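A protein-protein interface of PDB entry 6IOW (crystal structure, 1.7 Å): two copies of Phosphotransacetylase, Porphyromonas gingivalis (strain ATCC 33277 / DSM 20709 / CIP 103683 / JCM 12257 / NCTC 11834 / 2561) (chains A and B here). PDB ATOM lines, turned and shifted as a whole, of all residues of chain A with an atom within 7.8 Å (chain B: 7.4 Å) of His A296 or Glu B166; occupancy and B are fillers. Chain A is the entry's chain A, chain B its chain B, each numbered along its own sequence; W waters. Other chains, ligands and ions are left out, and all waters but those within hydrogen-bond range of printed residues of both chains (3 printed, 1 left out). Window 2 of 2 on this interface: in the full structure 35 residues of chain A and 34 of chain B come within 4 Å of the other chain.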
ATOM      1  N   LEU A   3      18.546  39.247  -1.598  1.00  0.00           N
ATOM      2  CA  LEU A   3      19.809  39.932  -1.862  1.00  0.00           C
ATOM      3  C   LEU A   3      19.587  41.071  -2.871  1.00  0.00           C
ATOM      4  O   LEU A   3      20.112  42.162  -2.690  1.00  0.00           O
ATOM      5  CB  LEU A   3      20.850  38.930  -2.378  1.00  0.00           C
ATOM      6  CG  LEU A   3      21.189  37.762  -1.448  1.00  0.00           C
ATOM      7  CD1 LEU A   3      22.122  36.772  -2.129  1.00  0.00           C
ATOM      8  CD2 LEU A   3      21.802  38.262  -0.148  1.00  0.00           C
ATOM      9  N   LEU A 160      25.620  40.475  -9.850  1.00  0.00           N
ATOM     10  CA  LEU A 160      25.922  39.361  -8.983  1.00  0.00           C
ATOM     11  C   LEU A 160      25.799  39.860  -7.544  1.00  0.00           C
ATOM     12  O   LEU A 160      26.691  40.531  -7.018  1.00  0.00           O
ATOM     13  CB  LEU A 160      27.324  38.837  -9.312  1.00  0.00           C
ATOM     14  CG  LEU A 160      27.686  37.449  -8.791  1.00  0.00           C
ATOM     15  CD1 LEU A 160      26.731  36.387  -9.307  1.00  0.00           C
ATOM     16  CD2 LEU A 160      29.114  37.096  -9.166  1.00  0.00           C
ATOM     17  N   PHE A 161      24.646  39.562  -6.941  1.00  0.00           N
ATOM     18  CA  PHE A 161      24.368  39.903  -5.562  1.00  0.00           C
ATOM     19  C   PHE A 161      24.883  38.768  -4.673  1.00  0.00           C
ATOM     20  O   PHE A 161      24.222  37.730  -4.526  1.00  0.00           O
ATOM     21  CB  PHE A 161      22.867  40.101  -5.352  1.00  0.00           C
ATOM     22  CG  PHE A 161      22.252  41.249  -6.113  1.00  0.00           C
ATOM     23  CD1 PHE A 161      22.312  42.539  -5.602  1.00  0.00           C
ATOM     24  CD2 PHE A 161      21.609  41.053  -7.324  1.00  0.00           C
ATOM     25  CE1 PHE A 161      21.733  43.603  -6.281  1.00  0.00           C
ATOM     26  CE2 PHE A 161      21.042  42.120  -8.007  1.00  0.00           C
ATOM     27  CZ  PHE A 161      21.096  43.390  -7.479  1.00  0.00           C
ATOM     28  N   THR A 162      26.066  38.979  -4.091  1.00  0.00           N
ATOM     29  CA  THR A 162      26.736  37.942  -3.294  1.00  0.00           C
ATOM     30  C   THR A 162      26.364  38.105  -1.817  1.00  0.00           C
ATOM     31  O   THR A 162      25.836  39.133  -1.407  1.00  0.00           O
ATOM     32  CB  THR A 162      28.259  37.971  -3.475  1.00  0.00           C
ATOM     33  OG1 THR A 162      28.803  39.027  -2.682  1.00  0.00           O
ATOM     34  CG2 THR A 162      28.669  38.135  -4.923  1.00  0.00           C
ATOM     35  N   LYS A 163      26.673  37.064  -1.041  1.00  0.00           N
ATOM     36  CA  LYS A 163      26.468  37.044   0.400  1.00  0.00           C
ATOM     37  C   LYS A 163      27.699  37.601   1.127  1.00  0.00           C
ATOM     38  O   LYS A 163      27.724  37.618   2.358  1.00  0.00           O
ATOM     39  CB  LYS A 163      26.125  35.619   0.846  1.00  0.00           C
ATOM     40  CG  LYS A 163      24.769  35.130   0.357  1.00  0.00           C
ATOM     41  CD  LYS A 163      24.386  33.755   0.836  1.00  0.00           C
ATOM     42  CE  LYS A 163      24.243  33.665   2.339  1.00  0.00           C
ATOM     43  NZ  LYS A 163      23.528  32.428   2.737  1.00  0.00           N
ATOM     44  N   LYS A 289      28.423  31.367 -12.734  1.00  0.00           N
ATOM     45  CA  LYS A 289      27.552  30.229 -12.412  1.00  0.00           C
ATOM     46  C   LYS A 289      28.036  29.530 -11.127  1.00  0.00           C
ATOM     47  O   LYS A 289      27.220  29.148 -10.294  1.00  0.00           O
ATOM     48  CB  LYS A 289      27.478  29.248 -13.588  1.00  0.00           C
ATOM     49  CG  LYS A 289      26.623  29.700 -14.765  1.00  0.00           C
ATOM     50  CD  LYS A 289      26.617  28.686 -15.901  1.00  0.00           C
ATOM     51  CE  LYS A 289      26.044  29.216 -17.197  1.00  0.00           C
ATOM     52  NZ  LYS A 289      24.600  29.502 -17.068  1.00  0.00           N
ATOM     53  N   LEU A 290      29.353  29.372 -10.956  1.00  0.00           N
ATOM     54  CA  LEU A 290      29.885  28.748  -9.730  1.00  0.00           C
ATOM     55  C   LEU A 290      29.651  29.658  -8.516  1.00  0.00           C
ATOM     56  O   LEU A 290      29.330  29.162  -7.441  1.00  0.00           O
ATOM     57  CB  LEU A 290      31.373  28.425  -9.888  1.00  0.00           C
ATOM     58  CG  LEU A 290      31.711  27.311 -10.877  1.00  0.00           C
ATOM     59  CD1 LEU A 290      33.210  27.064 -10.904  1.00  0.00           C
ATOM     60  CD2 LEU A 290      30.967  26.032 -10.532  1.00  0.00           C
ATOM     61  N   VAL A 291      29.793  30.978  -8.680  1.00  0.00           N
ATOM     62  CA  VAL A 291      29.527  31.883  -7.554  1.00  0.00           C
ATOM     63  C   VAL A 291      28.039  31.795  -7.184  1.00  0.00           C
ATOM     64  O   VAL A 291      27.688  31.762  -6.010  1.00  0.00           O
ATOM     65  CB  VAL A 291      29.980  33.325  -7.842  1.00  0.00           C
ATOM     66  CG1 VAL A 291      29.537  34.276  -6.734  1.00  0.00           C
ATOM     67  CG2 VAL A 291      31.488  33.409  -8.038  1.00  0.00           C
ATOM     68  N   GLU A 292      27.168  31.742  -8.198  1.00  0.00           N
ATOM     69  CA  GLU A 292      25.723  31.587  -8.002  1.00  0.00           C
ATOM     70  C   GLU A 292      25.420  30.289  -7.238  1.00  0.00           C
ATOM     71  O   GLU A 292      24.774  30.321  -6.181  1.00  0.00           O
ATOM     72  CB  GLU A 292      25.018  31.607  -9.360  1.00  0.00           C
ATOM     73  CG  GLU A 292      23.509  31.538  -9.282  1.00  0.00           C
ATOM     74  CD  GLU A 292      22.808  31.517 -10.627  1.00  0.00           C
ATOM     75  OE1 GLU A 292      23.499  31.444 -11.662  1.00  0.00           O
ATOM     76  OE2 GLU A 292      21.561  31.545 -10.637  1.00  0.00           O
ATOM     77  N   ARG A 293      25.906  29.153  -7.754  1.00  0.00           N
ATOM     78  CA  ARG A 293      25.503  27.832  -7.247  1.00  0.00           C
ATOM     79  C   ARG A 293      26.253  27.497  -5.951  1.00  0.00           C
ATOM     80  O   ARG A 293      25.610  27.175  -4.945  1.00  0.00           O
ATOM     81  CB  ARG A 293      25.695  26.757  -8.324  1.00  0.00           C
ATOM     82  CG  ARG A 293      24.826  26.953  -9.559  1.00  0.00           C
ATOM     83  CD  ARG A 293      23.338  26.921  -9.270  1.00  0.00           C
ATOM     84  NE  ARG A 293      22.552  27.116 -10.483  1.00  0.00           N
ATOM     85  CZ  ARG A 293      21.260  26.827 -10.584  1.00  0.00           C
ATOM     86  NH1 ARG A 293      20.602  26.372  -9.529  1.00  0.00           N
ATOM     87  NH2 ARG A 293      20.633  26.989 -11.736  1.00  0.00           N
ATOM     88  N   LEU A 294      27.589  27.579  -5.967  1.00  0.00           N
ATOM     89  CA  LEU A 294      28.396  27.187  -4.798  1.00  0.00           C
ATOM     90  C   LEU A 294      28.362  28.290  -3.732  1.00  0.00           C
ATOM     91  O   LEU A 294      28.534  27.995  -2.548  1.00  0.00           O
ATOM     92  CB  LEU A 294      29.831  26.870  -5.220  1.00  0.00           C
ATOM     93  CG  LEU A 294      29.997  25.718  -6.213  1.00  0.00           C
ATOM     94  CD1 LEU A 294      31.465  25.500  -6.566  1.00  0.00           C
ATOM     95  CD2 LEU A 294      29.390  24.437  -5.662  1.00  0.00           C
ATOM     96  N   GLY A 295      28.132  29.546  -4.144  1.00  0.00           N
ATOM     97  CA  GLY A 295      28.207  30.696  -3.236  1.00  0.00           C
ATOM     98  C   GLY A 295      26.854  31.222  -2.787  1.00  0.00           C
ATOM     99  O   GLY A 295      26.799  32.116  -1.939  1.00  0.00           O
ATOM    100  N   HIS A 296      25.771  30.684  -3.357  1.00  0.00           N
ATOM    101  CA  HIS A 296      24.389  31.114  -3.090  1.00  0.00           C
ATOM    102  C   HIS A 296      24.194  32.594  -3.453  1.00  0.00           C
ATOM    103  O   HIS A 296      23.395  33.287  -2.836  1.00  0.00           O
ATOM    104  CB  HIS A 296      23.986  30.828  -1.631  1.00  0.00           C
ATOM    105  CG  HIS A 296      23.822  29.377  -1.321  1.00  0.00           C
ATOM    106  ND1 HIS A 296      24.231  28.832  -0.118  1.00  0.00           N
ATOM    107  CD2 HIS A 296      23.311  28.358  -2.042  1.00  0.00           C
ATOM    108  CE1 HIS A 296      23.975  27.543  -0.114  1.00  0.00           C
ATOM    109  NE2 HIS A 296      23.405  27.224  -1.276  1.00  0.00           N
ATOM    110  N   ALA A 297      24.925  33.078  -4.460  1.00  0.00           N
ATOM    111  CA  ALA A 297      24.732  34.441  -4.949  1.00  0.00           C
ATOM    112  C   ALA A 297      23.513  34.462  -5.877  1.00  0.00           C
ATOM    113  O   ALA A 297      23.170  33.447  -6.478  1.00  0.00           O
ATOM    114  CB  ALA A 297      25.977  34.927  -5.650  1.00  0.00           C
ATOM    115  N   GLU A 298      22.851  35.617  -5.954  1.00  0.00           N
ATOM    116  CA  GLU A 298      21.761  35.829  -6.893  1.00  0.00           C
ATOM    117  C   GLU A 298      22.326  36.534  -8.125  1.00  0.00           C
ATOM    118  O   GLU A 298      22.983  37.563  -7.993  1.00  0.00           O
ATOM    119  CB  GLU A 298      20.653  36.658  -6.249  1.00  0.00           C
ATOM    120  CG  GLU A 298      19.897  35.906  -5.178  1.00  0.00           C
ATOM    121  CD  GLU A 298      19.002  36.795  -4.339  1.00  0.00           C
ATOM    122  OE1 GLU A 298      18.751  37.941  -4.762  1.00  0.00           O
ATOM    123  OE2 GLU A 298      18.570  36.344  -3.259  1.00  0.00           O
ATOM    124  N   ALA A 299      22.073  35.956  -9.303  1.00  0.00           N
ATOM    125  CA  ALA A 299      22.603  36.473 -10.572  1.00  0.00           C
ATOM    126  C   ALA A 299      21.430  36.979 -11.417  1.00  0.00           C
ATOM    127  O   ALA A 299      20.644  36.180 -11.901  1.00  0.00           O
ATOM    128  CB  ALA A 299      23.391  35.394 -11.286  1.00  0.00           C
ATOM    129  N   THR B 162      32.665  24.352   0.229  1.00  0.00           N
ATOM    130  CA  THR B 162      31.640  25.363  -0.046  1.00  0.00           C
ATOM    131  C   THR B 162      30.523  25.280   0.996  1.00  0.00           C
ATOM    132  O   THR B 162      30.404  24.295   1.726  1.00  0.00           O
ATOM    133  CB  THR B 162      31.053  25.219  -1.459  1.00  0.00           C
ATOM    134  OG1 THR B 162      30.082  24.169  -1.476  1.00  0.00           O
ATOM    135  CG2 THR B 162      32.119  24.971  -2.503  1.00  0.00           C
ATOM    136  N   LYS B 163      29.689  26.328   1.030  1.00  0.00           N
ATOM    137  CA  LYS B 163      28.537  26.405   1.919  1.00  0.00           C
ATOM    138  C   LYS B 163      27.294  25.814   1.242  1.00  0.00           C
ATOM    139  O   LYS B 163      26.204  25.859   1.804  1.00  0.00           O
ATOM    140  CB  LYS B 163      28.325  27.858   2.352  1.00  0.00           C
ATOM    141  CG  LYS B 163      29.393  28.381   3.301  1.00  0.00           C
ATOM    142  CD  LYS B 163      29.174  29.816   3.701  1.00  0.00           C
ATOM    143  CE  LYS B 163      29.667  30.137   5.099  1.00  0.00           C
ATOM    144  NZ  LYS B 163      29.093  31.410   5.602  1.00  0.00           N
ATOM    145  N   ALA B 164      27.468  25.233   0.048  1.00  0.00           N
ATOM    146  CA  ALA B 164      26.384  24.579  -0.678  1.00  0.00           C
ATOM    147  C   ALA B 164      26.512  23.061  -0.512  1.00  0.00           C
ATOM    148  O   ALA B 164      27.013  22.372  -1.384  1.00  0.00           O
ATOM    149  CB  ALA B 164      26.417  25.001  -2.129  1.00  0.00           C
ATOM    150  N   LYS B 165      26.029  22.552   0.628  1.00  0.00           N
ATOM    151  CA  LYS B 165      26.220  21.153   1.016  1.00  0.00           C
ATOM    152  C   LYS B 165      25.475  20.210   0.058  1.00  0.00           C
ATOM    153  O   LYS B 165      25.770  19.024   0.030  1.00  0.00           O
ATOM    154  CB  LYS B 165      25.775  20.936   2.468  1.00  0.00           C
ATOM    155  CG  LYS B 165      26.710  21.510   3.524  1.00  0.00           C
ATOM    156  CD  LYS B 165      26.416  20.990   4.924  1.00  0.00           C
ATOM    157  CE  LYS B 165      27.240  21.661   6.002  1.00  0.00           C
ATOM    158  NZ  LYS B 165      28.658  21.232   5.954  1.00  0.00           N
ATOM    159  N   GLU B 166      24.536  20.742  -0.735  1.00  0.00           N
ATOM    160  CA  GLU B 166      23.767  19.954  -1.701  1.00  0.00           C
ATOM    161  C   GLU B 166      24.637  19.575  -2.913  1.00  0.00           C
ATOM    162  O   GLU B 166      24.218  18.745  -3.716  1.00  0.00           O
ATOM    163  CB  GLU B 166      22.485  20.684  -2.131  1.00  0.00           C
ATOM    164  CG  GLU B 166      22.697  21.945  -2.964  1.00  0.00           C
ATOM    165  CD  GLU B 166      22.880  23.230  -2.172  1.00  0.00           C
ATOM    166  OE1 GLU B 166      22.547  24.311  -2.697  1.00  0.00           O
ATOM    167  OE2 GLU B 166      23.360  23.145  -1.024  1.00  0.00           O
ATOM    168  N   TYR B 167      25.835  20.164  -3.035  1.00  0.00           N
ATOM    169  CA  TYR B 167      26.759  19.894  -4.151  1.00  0.00           C
ATOM    170  C   TYR B 167      28.041  19.226  -3.643  1.00  0.00           C
ATOM    171  O   TYR B 167      28.404  19.356  -2.471  1.00  0.00           O
ATOM    172  CB  TYR B 167      27.091  21.182  -4.903  1.00  0.00           C
ATOM    173  CG  TYR B 167      25.888  21.903  -5.444  1.00  0.00           C
ATOM    174  CD1 TYR B 167      24.975  21.259  -6.261  1.00  0.00           C
ATOM    175  CD2 TYR B 167      25.658  23.234  -5.137  1.00  0.00           C
ATOM    176  CE1 TYR B 167      23.861  21.919  -6.755  1.00  0.00           C
ATOM    177  CE2 TYR B 167      24.550  23.907  -5.626  1.00  0.00           C
ATOM    178  CZ  TYR B 167      23.656  23.253  -6.450  1.00  0.00           C
ATOM    179  OH  TYR B 167      22.569  23.911  -6.943  1.00  0.00           O
ATOM    180  N   GLY B 168      28.715  18.507  -4.550  1.00  0.00           N
ATOM    181  CA  GLY B 168      29.895  17.725  -4.227  1.00  0.00           C
ATOM    182  C   GLY B 168      29.623  16.742  -3.095  1.00  0.00           C
ATOM    183  O   GLY B 168      28.552  16.162  -3.016  1.00  0.00           O
ATOM    184  N   LYS B 169      30.607  16.573  -2.210  1.00  0.00           N
ATOM    185  CA  LYS B 169      30.466  15.736  -1.023  1.00  0.00           C
ATOM    186  C   LYS B 169      30.326  16.649   0.200  1.00  0.00           C
ATOM    187  O   LYS B 169      31.321  17.140   0.719  1.00  0.00           O
ATOM    188  CB  LYS B 169      31.674  14.807  -0.878  1.00  0.00           C
ATOM    189  CG  LYS B 169      31.594  13.858   0.308  1.00  0.00           C
ATOM    190  CD  LYS B 169      32.813  12.971   0.479  1.00  0.00           C
ATOM    191  CE  LYS B 169      32.657  12.026   1.656  1.00  0.00           C
ATOM    192  NZ  LYS B 169      33.897  11.255   1.915  1.00  0.00           N
ATOM    193  N   ASP B 170      29.079  16.871   0.624  1.00  0.00           N
ATOM    194  CA  ASP B 170      28.733  17.781   1.732  1.00  0.00           C
ATOM    195  C   ASP B 170      29.380  19.149   1.488  1.00  0.00           C
ATOM    196  O   ASP B 170      29.932  19.770   2.409  1.00  0.00           O
ATOM    197  CB  ASP B 170      29.162  17.210   3.092  1.00  0.00           C
ATOM    198  CG  ASP B 170      28.646  15.812   3.361  1.00  0.00           C
ATOM    199  OD1 ASP B 170      27.416  15.638   3.353  1.00  0.00           O
ATOM    200  OD2 ASP B 170      29.483  14.906   3.558  1.00  0.00           O
ATOM    201  N   GLY B 171      29.338  19.604   0.229  1.00  0.00           N
ATOM    202  CA  GLY B 171      29.815  20.928  -0.137  1.00  0.00           C
ATOM    203  C   GLY B 171      31.247  20.944  -0.650  1.00  0.00           C
ATOM    204  O   GLY B 171      31.673  21.961  -1.162  1.00  0.00           O
ATOM    205  N   LEU B 255      26.430  20.795 -11.922  1.00  0.00           N
ATOM    206  CA  LEU B 255      25.980  20.791 -10.521  1.00  0.00           C
ATOM    207  C   LEU B 255      24.469  20.541 -10.384  1.00  0.00           C
ATOM    208  O   LEU B 255      24.043  19.998  -9.352  1.00  0.00           O
ATOM    209  CB  LEU B 255      26.353  22.127  -9.868  1.00  0.00           C
ATOM    210  CG  LEU B 255      27.843  22.444  -9.738  1.00  0.00           C
ATOM    211  CD1 LEU B 255      28.037  23.803  -9.073  1.00  0.00           C
ATOM    212  CD2 LEU B 255      28.601  21.366  -8.974  1.00  0.00           C
ATOM    213  N   GLY B 271      25.048  16.920 -13.241  1.00  0.00           N
ATOM    214  CA  GLY B 271      24.064  16.996 -12.168  1.00  0.00           C
ATOM    215  C   GLY B 271      24.570  16.454 -10.843  1.00  0.00           C
ATOM    216  O   GLY B 271      23.840  16.564  -9.852  1.00  0.00           O
ATOM    217  N   LYS B 272      25.770  15.864 -10.810  1.00  0.00           N
ATOM    218  CA  LYS B 272      26.329  15.391  -9.537  1.00  0.00           C
ATOM    219  C   LYS B 272      27.861  15.432  -9.543  1.00  0.00           C
ATOM    220  O   LYS B 272      28.522  14.630  -8.888  1.00  0.00           O
ATOM    221  CB  LYS B 272      25.785  13.992  -9.237  1.00  0.00           C
ATOM    222  CG  LYS B 272      25.924  12.988 -10.369  1.00  0.00           C
ATOM    223  CD  LYS B 272      24.993  11.789 -10.272  1.00  0.00           C
ATOM    224  CE  LYS B 272      25.050  10.892 -11.493  1.00  0.00           C
ATOM    225  NZ  LYS B 272      24.896  11.662 -12.757  1.00  0.00           N
ATOM    226  N   ALA B 273      28.437  16.414 -10.243  1.00  0.00           N
ATOM    227  CA  ALA B 273      29.893  16.562 -10.327  1.00  0.00           C
ATOM    228  C   ALA B 273      30.474  16.886  -8.945  1.00  0.00           C
ATOM    229  O   ALA B 273      29.900  17.678  -8.206  1.00  0.00           O
ATOM    230  CB  ALA B 273      30.243  17.649 -11.311  1.00  0.00           C
ATOM    231  N   LEU B 294      33.726  35.479  -2.733  1.00  0.00           N
ATOM    232  CA  LEU B 294      32.334  35.902  -2.891  1.00  0.00           C
ATOM    233  C   LEU B 294      31.365  34.835  -2.362  1.00  0.00           C
ATOM    234  O   LEU B 294      30.240  35.159  -2.013  1.00  0.00           O
ATOM    235  CB  LEU B 294      32.064  36.226  -4.366  1.00  0.00           C
ATOM    236  CG  LEU B 294      32.906  37.347  -4.978  1.00  0.00           C
ATOM    237  CD1 LEU B 294      32.498  37.590  -6.427  1.00  0.00           C
ATOM    238  CD2 LEU B 294      32.765  38.635  -4.181  1.00  0.00           C
ATOM    239  N   GLY B 295      31.804  33.569  -2.305  1.00  0.00           N
ATOM    240  CA  GLY B 295      30.948  32.446  -1.891  1.00  0.00           C
ATOM    241  C   GLY B 295      31.178  31.992  -0.453  1.00  0.00           C
ATOM    242  O   GLY B 295      30.444  31.137   0.048  1.00  0.00           O
HETATM  243  O   HOH W   1      27.727  31.630   0.705  1.00  0.00           O
HETATM  244  O   HOH W   2      27.552  34.638  -2.472  1.00  0.00           O
HETATM  245  O   HOH W   3      30.564  28.486  -0.746  1.00  0.00           O
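NE2 of His A296 sits at hydrogen-bond distance from OE1 of Glu B166, 3.4 Å away.
The backbone carbonyl oxygen of Gly B171 is in hydrogen-bond range of the side-chain hydroxyl of Thr B162, 2.7 Å away. The backbone NH (N) of Ala A297 lies within hydrogen-bond range of the backbone carbonyl oxygen (O) of Val A291, at 3.4 Å. OG1 of Thr B162 sits close to N of Ala B164, at 3.2 Å. The backbone NH (N) of His A296 sits at hydrogen-bond distance from the backbone carbonyl oxygen (O) of Val A291 (3.4 Å).
Among the printed residues, pairs that only touch across the chains: Thr A162 with Leu B294 (3.7 Å), Leu A290 with Leu B255 (3.96 Å), Val A291 with Leu B294 (3.97 Å), Arg A293 with Ala B164 (3.6 Å), Arg A293 with Tyr B167 (3.5 Å), Arg A293 with Leu B255 (3.8 Å), Leu A294 with Thr B162 (3.9 Å), Leu A294 with Ala B164 (3.7 Å), Leu A294 with Tyr B167 (3.96 Å), Leu A294 with Leu B255 (3.7 Å), Gly A295 with Gly B295 (3.5 Å), His A296 with Lys B163 (3.4 Å) and His A296 with Ala B164 (3.8 Å).
Of chain B, only Lys B163, Ala B164 and Glu B166 come within 4 Å of His A296. Glu B166 touches just one residue of chain A: His A296 (3.4 Å). Of the printed residues of chain B, Arg A293 touches Ala B164, Tyr B167 and Leu B255. Of the printed residues of chain B, Leu A290 touches Leu B255 (3.96 Å). The nearest residue of chain A that does not touch Glu B166 is Arg A293 (4.8 Å). The nearest printed residue of chain A that does not touch Ala B164 is Gly A295 (5.3 Å).
Printed residues of chain A that touch a printed residue of chain B: Thr A162, Leu A290, Val A291, Arg A293, Leu A294, Gly A295 and His A296. Hydrophobic or aromatic side chains of chain B within 4 Å of the printed part of chain A: Ala B164, Tyr B167, Leu B255 and Leu B294. Among the printed residues, no Asp or Glu carboxylate lies within 4 Å of a Lys or Arg side-chain nitrogen of the other chain.
Thr A162 touches Leu B294, and with the chains exchanged Leu A294 touches Thr B162. Gly A295 touches its own counterpart, Gly B295.
Water W2 lies within hydrogen-bond range of the backbone carbonyl oxygen (O) of Gly A295 (2.7 Å), the backbone carbonyl oxygen (O) of Leu B294 (2.8 Å) and the backbone NH (N) of Lys A163 (3.0 Å). Water W3 lies within hydrogen-bond range of O of Leu A294 (2.8 Å), O of Gly B295 (2.8 Å) and N of Lys B163 (2.9 Å). Water W1 bridges the backbone carbonyl oxygen of Gly B295 (2.8 Å) and the backbone carbonyl oxygen of Gly A295 (2.8 Å).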
